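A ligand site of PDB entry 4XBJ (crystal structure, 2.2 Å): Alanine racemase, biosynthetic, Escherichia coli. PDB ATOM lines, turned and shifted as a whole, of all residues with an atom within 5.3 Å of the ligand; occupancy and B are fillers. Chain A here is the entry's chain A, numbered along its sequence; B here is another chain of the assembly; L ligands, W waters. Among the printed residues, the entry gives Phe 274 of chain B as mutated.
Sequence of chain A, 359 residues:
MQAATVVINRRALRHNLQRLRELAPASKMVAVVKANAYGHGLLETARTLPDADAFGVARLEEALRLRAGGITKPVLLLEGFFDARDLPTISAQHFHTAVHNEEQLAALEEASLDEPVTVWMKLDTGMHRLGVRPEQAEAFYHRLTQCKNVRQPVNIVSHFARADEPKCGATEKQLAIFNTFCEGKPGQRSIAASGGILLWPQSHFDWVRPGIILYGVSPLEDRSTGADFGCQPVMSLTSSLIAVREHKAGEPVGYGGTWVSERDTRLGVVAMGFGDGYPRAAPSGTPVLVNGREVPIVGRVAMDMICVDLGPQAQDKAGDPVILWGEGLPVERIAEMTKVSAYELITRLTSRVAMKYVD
An oxygen (O6) of the ligand is in hydrogen-bond range of the side-chain hydroxyl of Tyr 255 of chain B, 2.4 Å away.
An oxygen (O5) of the ligand lies within hydrogen-bond range of the side-chain hydroxyl (OH) of Tyr 38, 2.6 Å away.
O1 of the ligand sits at hydrogen-bond distance from OH of Tyr 343, 2.6 Å away.
O8 of the ligand is in salt-bridge range of NZ of Lys 34, at 2.6 Å.
The backbone NH (N) of Met 303 of chain B sits at hydrogen-bond distance from an oxygen (O7) of the ligand, 2.6 Å away.
An oxygen (O2) of the ligand sits at hydrogen-bond distance from the backbone NH (N) of Ser 194, at 2.7 Å.
The side-chain hydroxyl (OG) of Ser 194 is in hydrogen-bond range of an oxygen (O2) of the ligand (2.7 Å).
An oxygen (O6) of the ligand is in salt-bridge range of the guanidinium group (NH1) of Arg 129, at 2.7 Å.
The backbone NH of Ile 212 is in hydrogen-bond range of an oxygen (O5) of the ligand (2.8 Å).
A nitrogen (N1) of the ligand lies within hydrogen-bond range of the guanidinium group (NE) of Arg 209, 2.9 Å away.
The backbone NH of Gly 211 sits at hydrogen-bond distance from an oxygen (O2) of the ligand, at 2.9 Å.
The side-chain hydroxyl of Tyr 255 of chain B lies within hydrogen-bond range of a ring nitrogen (NE2) of His 159 (3.0 Å).
NZ of Lys 34 sits at hydrogen-bond distance from SD of Met 303 of chain B.
The side-chain carboxylate of Asp 304 of chain B is in salt-bridge range of the side-chain amino group of Lys 34 (3.8 Å).
The side-chain hydroxyl of Ser 194 sits at hydrogen-bond distance from the backbone NH of Ile 212.
The side-chain hydroxyl (OG) of Ser 194 lies within hydrogen-bond range of the backbone NH (N) of Ile 213.
NH2 of Arg 209 is in hydrogen-bond range of ND1 of His 159, at 3.2 Å.
The backbone carbonyl oxygen of Ala 302 of chain B sits at hydrogen-bond distance from the backbone NH of Phe 274 of chain B (3.1 Å).
O of Pro 210 is in hydrogen-bond range of N of Val 32 (2.9 Å).
OD2 of Asp 304 of chain B sits close to O8 of the ligand, 3.4 Å away.
Residues that only touch the ligand: Val 32, His 159, Ala 193, Pro 210 and Ala 302 of chain B.
Hydrophobic or aromatic side chains within 4 Å of the ligand: Val 32, Tyr 38, His 159, Ala 193, Ile 212, Tyr 343, Tyr 255 of chain B, Ala 302 of chain B and Met 303 of chain B.
16 residues have an atom within 4 Å of the ligand: Val 32, Lys 34, Tyr 38, Arg 129, His 159, Ala 193, Ser 194, Arg 209, Pro 210, Gly 211, Ile 212, Tyr 343, Tyr 255 of chain B, Ala 302 of chain B, Met 303 of chain B and Asp 304 of chain B.
The nearest printed residue that does not touch the ligand is Leu 78 (4.1 Å).
Water W4 bridges O8 of the ligand and N of Asp 304 of chain B.
Water W3 lies within hydrogen-bond range of an oxygen (O1) of the ligand (2.8 Å), the side-chain hydroxyl (OH) of Tyr 255 of chain B (3.0 Å) and a ring nitrogen (NE2) of His 159 (3.4 Å).
Water W2 lies within hydrogen-bond range of N of Gly 195 (2.7 Å), O1 of the ligand (2.9 Å) and N of Ser 194 (3.1 Å).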
ATOM      1  N   VAL A  32      11.296  18.693   9.907  1.00  0.00           N
ATOM      2  CA  VAL A  32      12.149  19.516  10.737  1.00  0.00           C
ATOM      3  C   VAL A  32      11.872  19.285  12.222  1.00  0.00           C
ATOM      4  O   VAL A  32      10.737  19.493  12.664  1.00  0.00           O
ATOM      5  CB  VAL A  32      11.946  21.022  10.387  1.00  0.00           C
ATOM      6  CG1 VAL A  32      12.843  21.890  11.240  1.00  0.00           C
ATOM      7  CG2 VAL A  32      12.274  21.256   8.921  1.00  0.00           C
ATOM      8  N   LYS A  34      14.485  19.825  14.836  1.00  0.00           N
ATOM      9  CA  LYS A  34      15.374  20.582  15.702  1.00  0.00           C
ATOM     10  C   LYS A  34      14.694  21.154  16.919  1.00  0.00           C
ATOM     11  O   LYS A  34      13.478  21.201  16.997  1.00  0.00           O
ATOM     12  CB  LYS A  34      16.004  21.714  14.916  1.00  0.00           C
ATOM     13  CG  LYS A  34      15.051  22.831  14.538  1.00  0.00           C
ATOM     14  CD  LYS A  34      15.467  23.410  13.189  1.00  0.00           C
ATOM     15  CE  LYS A  34      14.638  24.615  12.833  1.00  0.00           C
ATOM     16  NZ  LYS A  34      15.029  25.767  13.671  1.00  0.00           N
ATOM     17  N   TYR A  38      10.662  21.015  18.184  1.00  0.00           N
ATOM     18  CA  TYR A  38       9.842  22.175  18.512  1.00  0.00           C
ATOM     19  C   TYR A  38       9.084  21.995  19.809  1.00  0.00           C
ATOM     20  O   TYR A  38       7.947  22.525  19.944  1.00  0.00           O
ATOM     21  CB  TYR A  38       8.849  22.466  17.391  1.00  0.00           C
ATOM     22  CG  TYR A  38       9.405  23.169  16.154  1.00  0.00           C
ATOM     23  CD1 TYR A  38      10.709  22.930  15.707  1.00  0.00           C
ATOM     24  CD2 TYR A  38       8.584  23.974  15.379  1.00  0.00           C
ATOM     25  CE1 TYR A  38      11.136  23.442  14.491  1.00  0.00           C
ATOM     26  CE2 TYR A  38       9.014  24.478  14.175  1.00  0.00           C
ATOM     27  CZ  TYR A  38      10.288  24.228  13.733  1.00  0.00           C
ATOM     28  OH  TYR A  38      10.725  24.785  12.555  1.00  0.00           O
ATOM     29  N   LEU A  78      21.093  21.514   8.960  1.00  0.00           N
ATOM     30  CA  LEU A  78      20.608  22.730   8.286  1.00  0.00           C
ATOM     31  C   LEU A  78      21.607  23.865   8.295  1.00  0.00           C
ATOM     32  O   LEU A  78      21.572  24.731   7.431  1.00  0.00           O
ATOM     33  CB  LEU A  78      19.326  23.209   8.953  1.00  0.00           C
ATOM     34  CG  LEU A  78      18.121  22.289   8.797  1.00  0.00           C
ATOM     35  CD1 LEU A  78      16.992  22.712   9.746  1.00  0.00           C
ATOM     36  CD2 LEU A  78      17.667  22.249   7.336  1.00  0.00           C
ATOM     37  N   LYS A 122      24.076  26.164   0.527  1.00  0.00           N
ATOM     38  CA  LYS A 122      23.148  27.176   0.997  1.00  0.00           C
ATOM     39  C   LYS A 122      23.348  28.513   0.300  1.00  0.00           C
ATOM     40  O   LYS A 122      24.406  29.148   0.435  1.00  0.00           O
ATOM     41  CB  LYS A 122      23.263  27.374   2.509  1.00  0.00           C
ATOM     42  CG  LYS A 122      22.072  28.125   3.087  1.00  0.00           C
ATOM     43  CD  LYS A 122      22.129  28.225   4.611  1.00  0.00           C
ATOM     44  CE  LYS A 122      21.843  26.875   5.252  1.00  0.00           C
ATOM     45  NZ  LYS A 122      20.473  26.827   5.827  1.00  0.00           N
ATOM     46  N   ARG A 129      21.073  35.579   6.600  1.00  0.00           N
ATOM     47  CA  ARG A 129      21.433  34.918   7.826  1.00  0.00           C
ATOM     48  C   ARG A 129      22.614  33.990   7.586  1.00  0.00           C
ATOM     49  O   ARG A 129      23.765  34.364   7.873  1.00  0.00           O
ATOM     50  CB  ARG A 129      20.219  34.162   8.385  1.00  0.00           C
ATOM     51  CG  ARG A 129      20.424  33.651   9.799  1.00  0.00           C
ATOM     52  CD  ARG A 129      19.126  33.176  10.400  1.00  0.00           C
ATOM     53  NE  ARG A 129      18.591  32.006   9.712  1.00  0.00           N
ATOM     54  CZ  ARG A 129      17.480  31.374  10.080  1.00  0.00           C
ATOM     55  NH1 ARG A 129      16.797  31.794  11.152  1.00  0.00           N
ATOM     56  NH2 ARG A 129      17.091  30.290   9.419  1.00  0.00           N
ATOM     57  N   HIS A 159      16.079  29.514   2.057  1.00  0.00           N
ATOM     58  CA  HIS A 159      15.022  29.627   3.068  1.00  0.00           C
ATOM     59  C   HIS A 159      14.365  31.006   3.009  1.00  0.00           C
ATOM     60  O   HIS A 159      15.056  31.998   2.825  1.00  0.00           O
ATOM     61  CB  HIS A 159      15.598  29.336   4.440  1.00  0.00           C
ATOM     62  CG  HIS A 159      14.565  29.221   5.525  1.00  0.00           C
ATOM     63  ND1 HIS A 159      13.470  28.381   5.431  1.00  0.00           N
ATOM     64  CD2 HIS A 159      14.525  29.753   6.772  1.00  0.00           C
ATOM     65  CE1 HIS A 159      12.790  28.421   6.571  1.00  0.00           C
ATOM     66  NE2 HIS A 159      13.371  29.302   7.365  1.00  0.00           N
ATOM     67  N   ALA A 193       9.662  25.910   3.611  1.00  0.00           N
ATOM     68  CA  ALA A 193       9.298  25.382   4.892  1.00  0.00           C
ATOM     69  C   ALA A 193       7.777  25.464   5.002  1.00  0.00           C
ATOM     70  O   ALA A 193       7.088  25.483   3.982  1.00  0.00           O
ATOM     71  CB  ALA A 193       9.977  26.199   5.988  1.00  0.00           C
ATOM     72  N   SER A 194       7.231  25.553   6.222  1.00  0.00           N
ATOM     73  CA  SER A 194       5.775  25.490   6.404  1.00  0.00           C
ATOM     74  C   SER A 194       5.026  26.490   5.525  1.00  0.00           C
ATOM     75  O   SER A 194       4.028  26.149   4.873  1.00  0.00           O
ATOM     76  CB  SER A 194       5.397  25.728   7.861  1.00  0.00           C
ATOM     77  OG  SER A 194       5.758  24.632   8.671  1.00  0.00           O
ATOM     78  N   GLY A 195       5.498  27.733   5.505  1.00  0.00           N
ATOM     79  CA  GLY A 195       4.838  28.795   4.747  1.00  0.00           C
ATOM     80  C   GLY A 195       4.853  28.597   3.248  1.00  0.00           C
ATOM     81  O   GLY A 195       3.862  28.887   2.549  1.00  0.00           O
ATOM     82  N   ARG A 209      10.324  21.308   3.588  1.00  0.00           N
ATOM     83  CA  ARG A 209      10.859  21.147   4.925  1.00  0.00           C
ATOM     84  C   ARG A 209       9.891  21.647   5.986  1.00  0.00           C
ATOM     85  O   ARG A 209      10.112  22.675   6.603  1.00  0.00           O
ATOM     86  CB  ARG A 209      12.209  21.891   5.059  1.00  0.00           C
ATOM     87  CG  ARG A 209      13.121  21.766   3.848  1.00  0.00           C
ATOM     88  CD  ARG A 209      14.520  22.313   4.107  1.00  0.00           C
ATOM     89  NE  ARG A 209      14.526  23.753   4.315  1.00  0.00           N
ATOM     90  CZ  ARG A 209      14.505  24.669   3.345  1.00  0.00           C
ATOM     91  NH1 ARG A 209      14.511  24.303   2.061  1.00  0.00           N
ATOM     92  NH2 ARG A 209      14.476  25.960   3.648  1.00  0.00           N
ATOM     93  N   PRO A 210       8.825  20.890   6.245  1.00  0.00           N
ATOM     94  CA  PRO A 210       7.903  21.340   7.289  1.00  0.00           C
ATOM     95  C   PRO A 210       8.506  21.284   8.677  1.00  0.00           C
ATOM     96  O   PRO A 210       8.979  20.222   9.103  1.00  0.00           O
ATOM     97  CB  PRO A 210       6.725  20.365   7.186  1.00  0.00           C
ATOM     98  CG  PRO A 210       7.304  19.128   6.527  1.00  0.00           C
ATOM     99  CD  PRO A 210       8.409  19.606   5.624  1.00  0.00           C
ATOM    100  N   GLY A 211       8.442  22.411   9.383  1.00  0.00           N
ATOM    101  CA  GLY A 211       8.567  22.425  10.839  1.00  0.00           C
ATOM    102  C   GLY A 211       7.218  22.620  11.540  1.00  0.00           C
ATOM    103  O   GLY A 211       6.519  21.661  11.851  1.00  0.00           O
ATOM    104  N   ILE A 212       6.814  23.882  11.695  1.00  0.00           N
ATOM    105  CA  ILE A 212       5.693  24.206  12.576  1.00  0.00           C
ATOM    106  C   ILE A 212       4.390  23.536  12.165  1.00  0.00           C
ATOM    107  O   ILE A 212       3.728  22.965  13.018  1.00  0.00           O
ATOM    108  CB  ILE A 212       5.528  25.740  12.781  1.00  0.00           C
ATOM    109  CG1 ILE A 212       4.622  26.023  14.003  1.00  0.00           C
ATOM    110  CG2 ILE A 212       4.990  26.388  11.525  1.00  0.00           C
ATOM    111  CD1 ILE A 212       5.116  27.115  14.929  1.00  0.00           C
ATOM    112  N   ILE A 213       4.093  23.470  10.859  1.00  0.00           N
ATOM    113  CA  ILE A 213       2.844  22.891  10.406  1.00  0.00           C
ATOM    114  C   ILE A 213       2.785  21.364  10.640  1.00  0.00           C
ATOM    115  O   ILE A 213       1.716  20.799  10.874  1.00  0.00           O
ATOM    116  CB  ILE A 213       2.534  23.211   8.915  1.00  0.00           C
ATOM    117  CG1 ILE A 213       1.096  22.783   8.562  1.00  0.00           C
ATOM    118  CG2 ILE A 213       3.517  22.489   7.978  1.00  0.00           C
ATOM    119  CD1 ILE A 213       0.031  23.466   9.417  1.00  0.00           C
ATOM    120  N   PRO A 219       2.050  28.575  10.616  1.00  0.00           N
ATOM    121  CA  PRO A 219       3.238  29.415  10.574  1.00  0.00           C
ATOM    122  C   PRO A 219       2.918  30.900  10.522  1.00  0.00           C
ATOM    123  O   PRO A 219       3.817  31.696  10.576  1.00  0.00           O
ATOM    124  CB  PRO A 219       3.923  28.981   9.269  1.00  0.00           C
ATOM    125  CG  PRO A 219       2.818  28.497   8.400  1.00  0.00           C
ATOM    126  CD  PRO A 219       1.802  27.878   9.347  1.00  0.00           C
ATOM    127  N   TYR A 343       5.719  29.713  17.600  1.00  0.00           N
ATOM    128  CA  TYR A 343       6.974  28.969  17.525  1.00  0.00           C
ATOM    129  C   TYR A 343       7.658  28.893  18.869  1.00  0.00           C
ATOM    130  O   TYR A 343       8.223  27.859  19.247  1.00  0.00           O
ATOM    131  CB  TYR A 343       7.950  29.618  16.535  1.00  0.00           C
ATOM    132  CG  TYR A 343       7.660  29.433  15.061  1.00  0.00           C
ATOM    133  CD1 TYR A 343       6.879  30.349  14.371  1.00  0.00           C
ATOM    134  CD2 TYR A 343       8.307  28.439  14.322  1.00  0.00           C
ATOM    135  CE1 TYR A 343       6.711  30.256  13.000  1.00  0.00           C
ATOM    136  CE2 TYR A 343       8.098  28.281  12.982  1.00  0.00           C
ATOM    137  CZ  TYR A 343       7.329  29.215  12.303  1.00  0.00           C
ATOM    138  OH  TYR A 343       7.185  29.113  10.947  1.00  0.00           O
ATOM    139  N   TYR B 255      13.769  37.419   9.812  1.00  0.00           N
ATOM    140  CA  TYR B 255      12.368  37.220   9.426  1.00  0.00           C
ATOM    141  C   TYR B 255      11.683  38.570   9.335  1.00  0.00           C
ATOM    142  O   TYR B 255      11.955  39.449  10.144  1.00  0.00           O
ATOM    143  CB  TYR B 255      11.655  36.350  10.481  1.00  0.00           C
ATOM    144  CG  TYR B 255      11.994  34.895  10.369  1.00  0.00           C
ATOM    145  CD1 TYR B 255      11.740  34.189   9.183  1.00  0.00           C
ATOM    146  CD2 TYR B 255      12.667  34.232  11.386  1.00  0.00           C
ATOM    147  CE1 TYR B 255      12.134  32.869   9.033  1.00  0.00           C
ATOM    148  CE2 TYR B 255      13.027  32.912  11.251  1.00  0.00           C
ATOM    149  CZ  TYR B 255      12.758  32.236  10.078  1.00  0.00           C
ATOM    150  OH  TYR B 255      13.127  30.927   9.922  1.00  0.00           O
ATOM    151  N   PHE B 274      15.860  30.871  20.625  1.00  0.00           N
ATOM    152  CA  PHE B 274      14.797  30.685  21.581  1.00  0.00           C
ATOM    153  C   PHE B 274      14.528  29.201  21.852  1.00  0.00           C
ATOM    154  O   PHE B 274      14.061  28.845  22.939  1.00  0.00           O
ATOM    155  CB  PHE B 274      13.534  31.519  21.243  1.00  0.00           C
ATOM    156  CG  PHE B 274      12.874  31.174  19.947  1.00  0.00           C
ATOM    157  CD1 PHE B 274      12.157  29.984  19.802  1.00  0.00           C
ATOM    158  CD2 PHE B 274      12.929  32.046  18.873  1.00  0.00           C
ATOM    159  CE1 PHE B 274      11.519  29.682  18.616  1.00  0.00           C
ATOM    160  CE2 PHE B 274      12.292  31.743  17.678  1.00  0.00           C
ATOM    161  CZ  PHE B 274      11.591  30.564  17.555  1.00  0.00           C
ATOM    162  N   ALA B 302      15.994  34.095  16.286  1.00  0.00           N
ATOM    163  CA  ALA B 302      15.397  32.918  15.691  1.00  0.00           C
ATOM    164  C   ALA B 302      15.592  31.719  16.596  1.00  0.00           C
ATOM    165  O   ALA B 302      16.177  31.823  17.673  1.00  0.00           O
ATOM    166  CB  ALA B 302      16.037  32.660  14.314  1.00  0.00           C
ATOM    167  N   MET B 303      15.063  30.584  16.181  1.00  0.00           N
ATOM    168  CA  MET B 303      15.023  29.428  17.068  1.00  0.00           C
ATOM    169  C   MET B 303      16.404  28.915  17.448  1.00  0.00           C
ATOM    170  O   MET B 303      16.638  28.517  18.597  1.00  0.00           O
ATOM    171  CB  MET B 303      14.182  28.311  16.451  1.00  0.00           C
ATOM    172  CG  MET B 303      13.883  27.174  17.411  1.00  0.00           C
ATOM    173  SD  MET B 303      12.922  25.834  16.687  1.00  0.00           S
ATOM    174  CE  MET B 303      11.328  26.625  16.428  1.00  0.00           C
ATOM    175  N   ASP B 304      17.339  28.917  16.492  1.00  0.00           N
ATOM    176  CA  ASP B 304      18.691  28.346  16.700  1.00  0.00           C
ATOM    177  C   ASP B 304      19.839  29.338  16.457  1.00  0.00           C
ATOM    178  O   ASP B 304      21.016  29.032  16.702  1.00  0.00           O
ATOM    179  CB  ASP B 304      18.884  27.102  15.807  1.00  0.00           C
ATOM    180  CG  ASP B 304      17.648  26.231  15.732  1.00  0.00           C
ATOM    181  OD1 ASP B 304      17.170  25.801  16.805  1.00  0.00           O
ATOM    182  OD2 ASP B 304      17.141  25.962  14.607  1.00  0.00           O
HETATM  183  C1  LIG L   1      12.966  24.622   7.536  1.00  0.00           C
HETATM  184  C2  LIG L   1      15.079  25.775   7.613  1.00  0.00           C
HETATM  185  C3  LIG L   1      14.740  26.316   8.856  1.00  0.00           C
HETATM  186  O1  LIG L   1       8.697  27.627   9.507  1.00  0.00           O
HETATM  187  O2  LIG L   1       8.332  25.270   8.693  1.00  0.00           O
HETATM  188  C4  LIG L   1      11.266  24.819   9.340  1.00  0.00           C
HETATM  189  C5  LIG L   1      13.129  26.584  10.831  1.00  0.00           C
HETATM  190  C6  LIG L   1      12.498  28.611  12.139  1.00  0.00           C
HETATM  191  C7  LIG L   1      11.902  27.677  13.183  1.00  0.00           C
HETATM  192  N1  LIG L   1      14.196  24.926   6.934  1.00  0.00           N
HETATM  193  C8  LIG L   1      13.479  26.069   9.424  1.00  0.00           C
HETATM  194  C9  LIG L   1      12.614  25.168   8.775  1.00  0.00           C
HETATM  195  O3  LIG L   1      15.637  27.162   9.436  1.00  0.00           O
HETATM  196  C10 LIG L   1      16.380  26.092   6.931  1.00  0.00           C
HETATM  197  O4  LIG L   1      10.566  26.060   9.393  1.00  0.00           O
HETATM  198  N2  LIG L   1      12.744  27.976  10.830  1.00  0.00           N
HETATM  199  P1  LIG L   1       8.988  26.162   9.715  1.00  0.00           P
HETATM  200  O5  LIG L   1       8.805  25.705  11.143  1.00  0.00           O
HETATM  201  P2  LIG L   1      14.035  29.387  12.763  1.00  0.00           P
HETATM  202  O6  LIG L   1      14.658  30.192  11.679  1.00  0.00           O
HETATM  203  O7  LIG L   1      13.709  30.287  13.962  1.00  0.00           O
HETATM  204  O8  LIG L   1      15.026  28.288  13.207  1.00  0.00           O
HETATM  205  O   HOH W   1      18.128  26.691  10.014  1.00  0.00           O
HETATM  206  O   HOH W   2       7.532  28.518   7.018  1.00  0.00           O
HETATM  207  O   HOH W   3      10.499  29.665   9.098  1.00  0.00           O
HETATM  208  O   HOH W   4      17.296  29.086  13.605  1.00  0.00           O
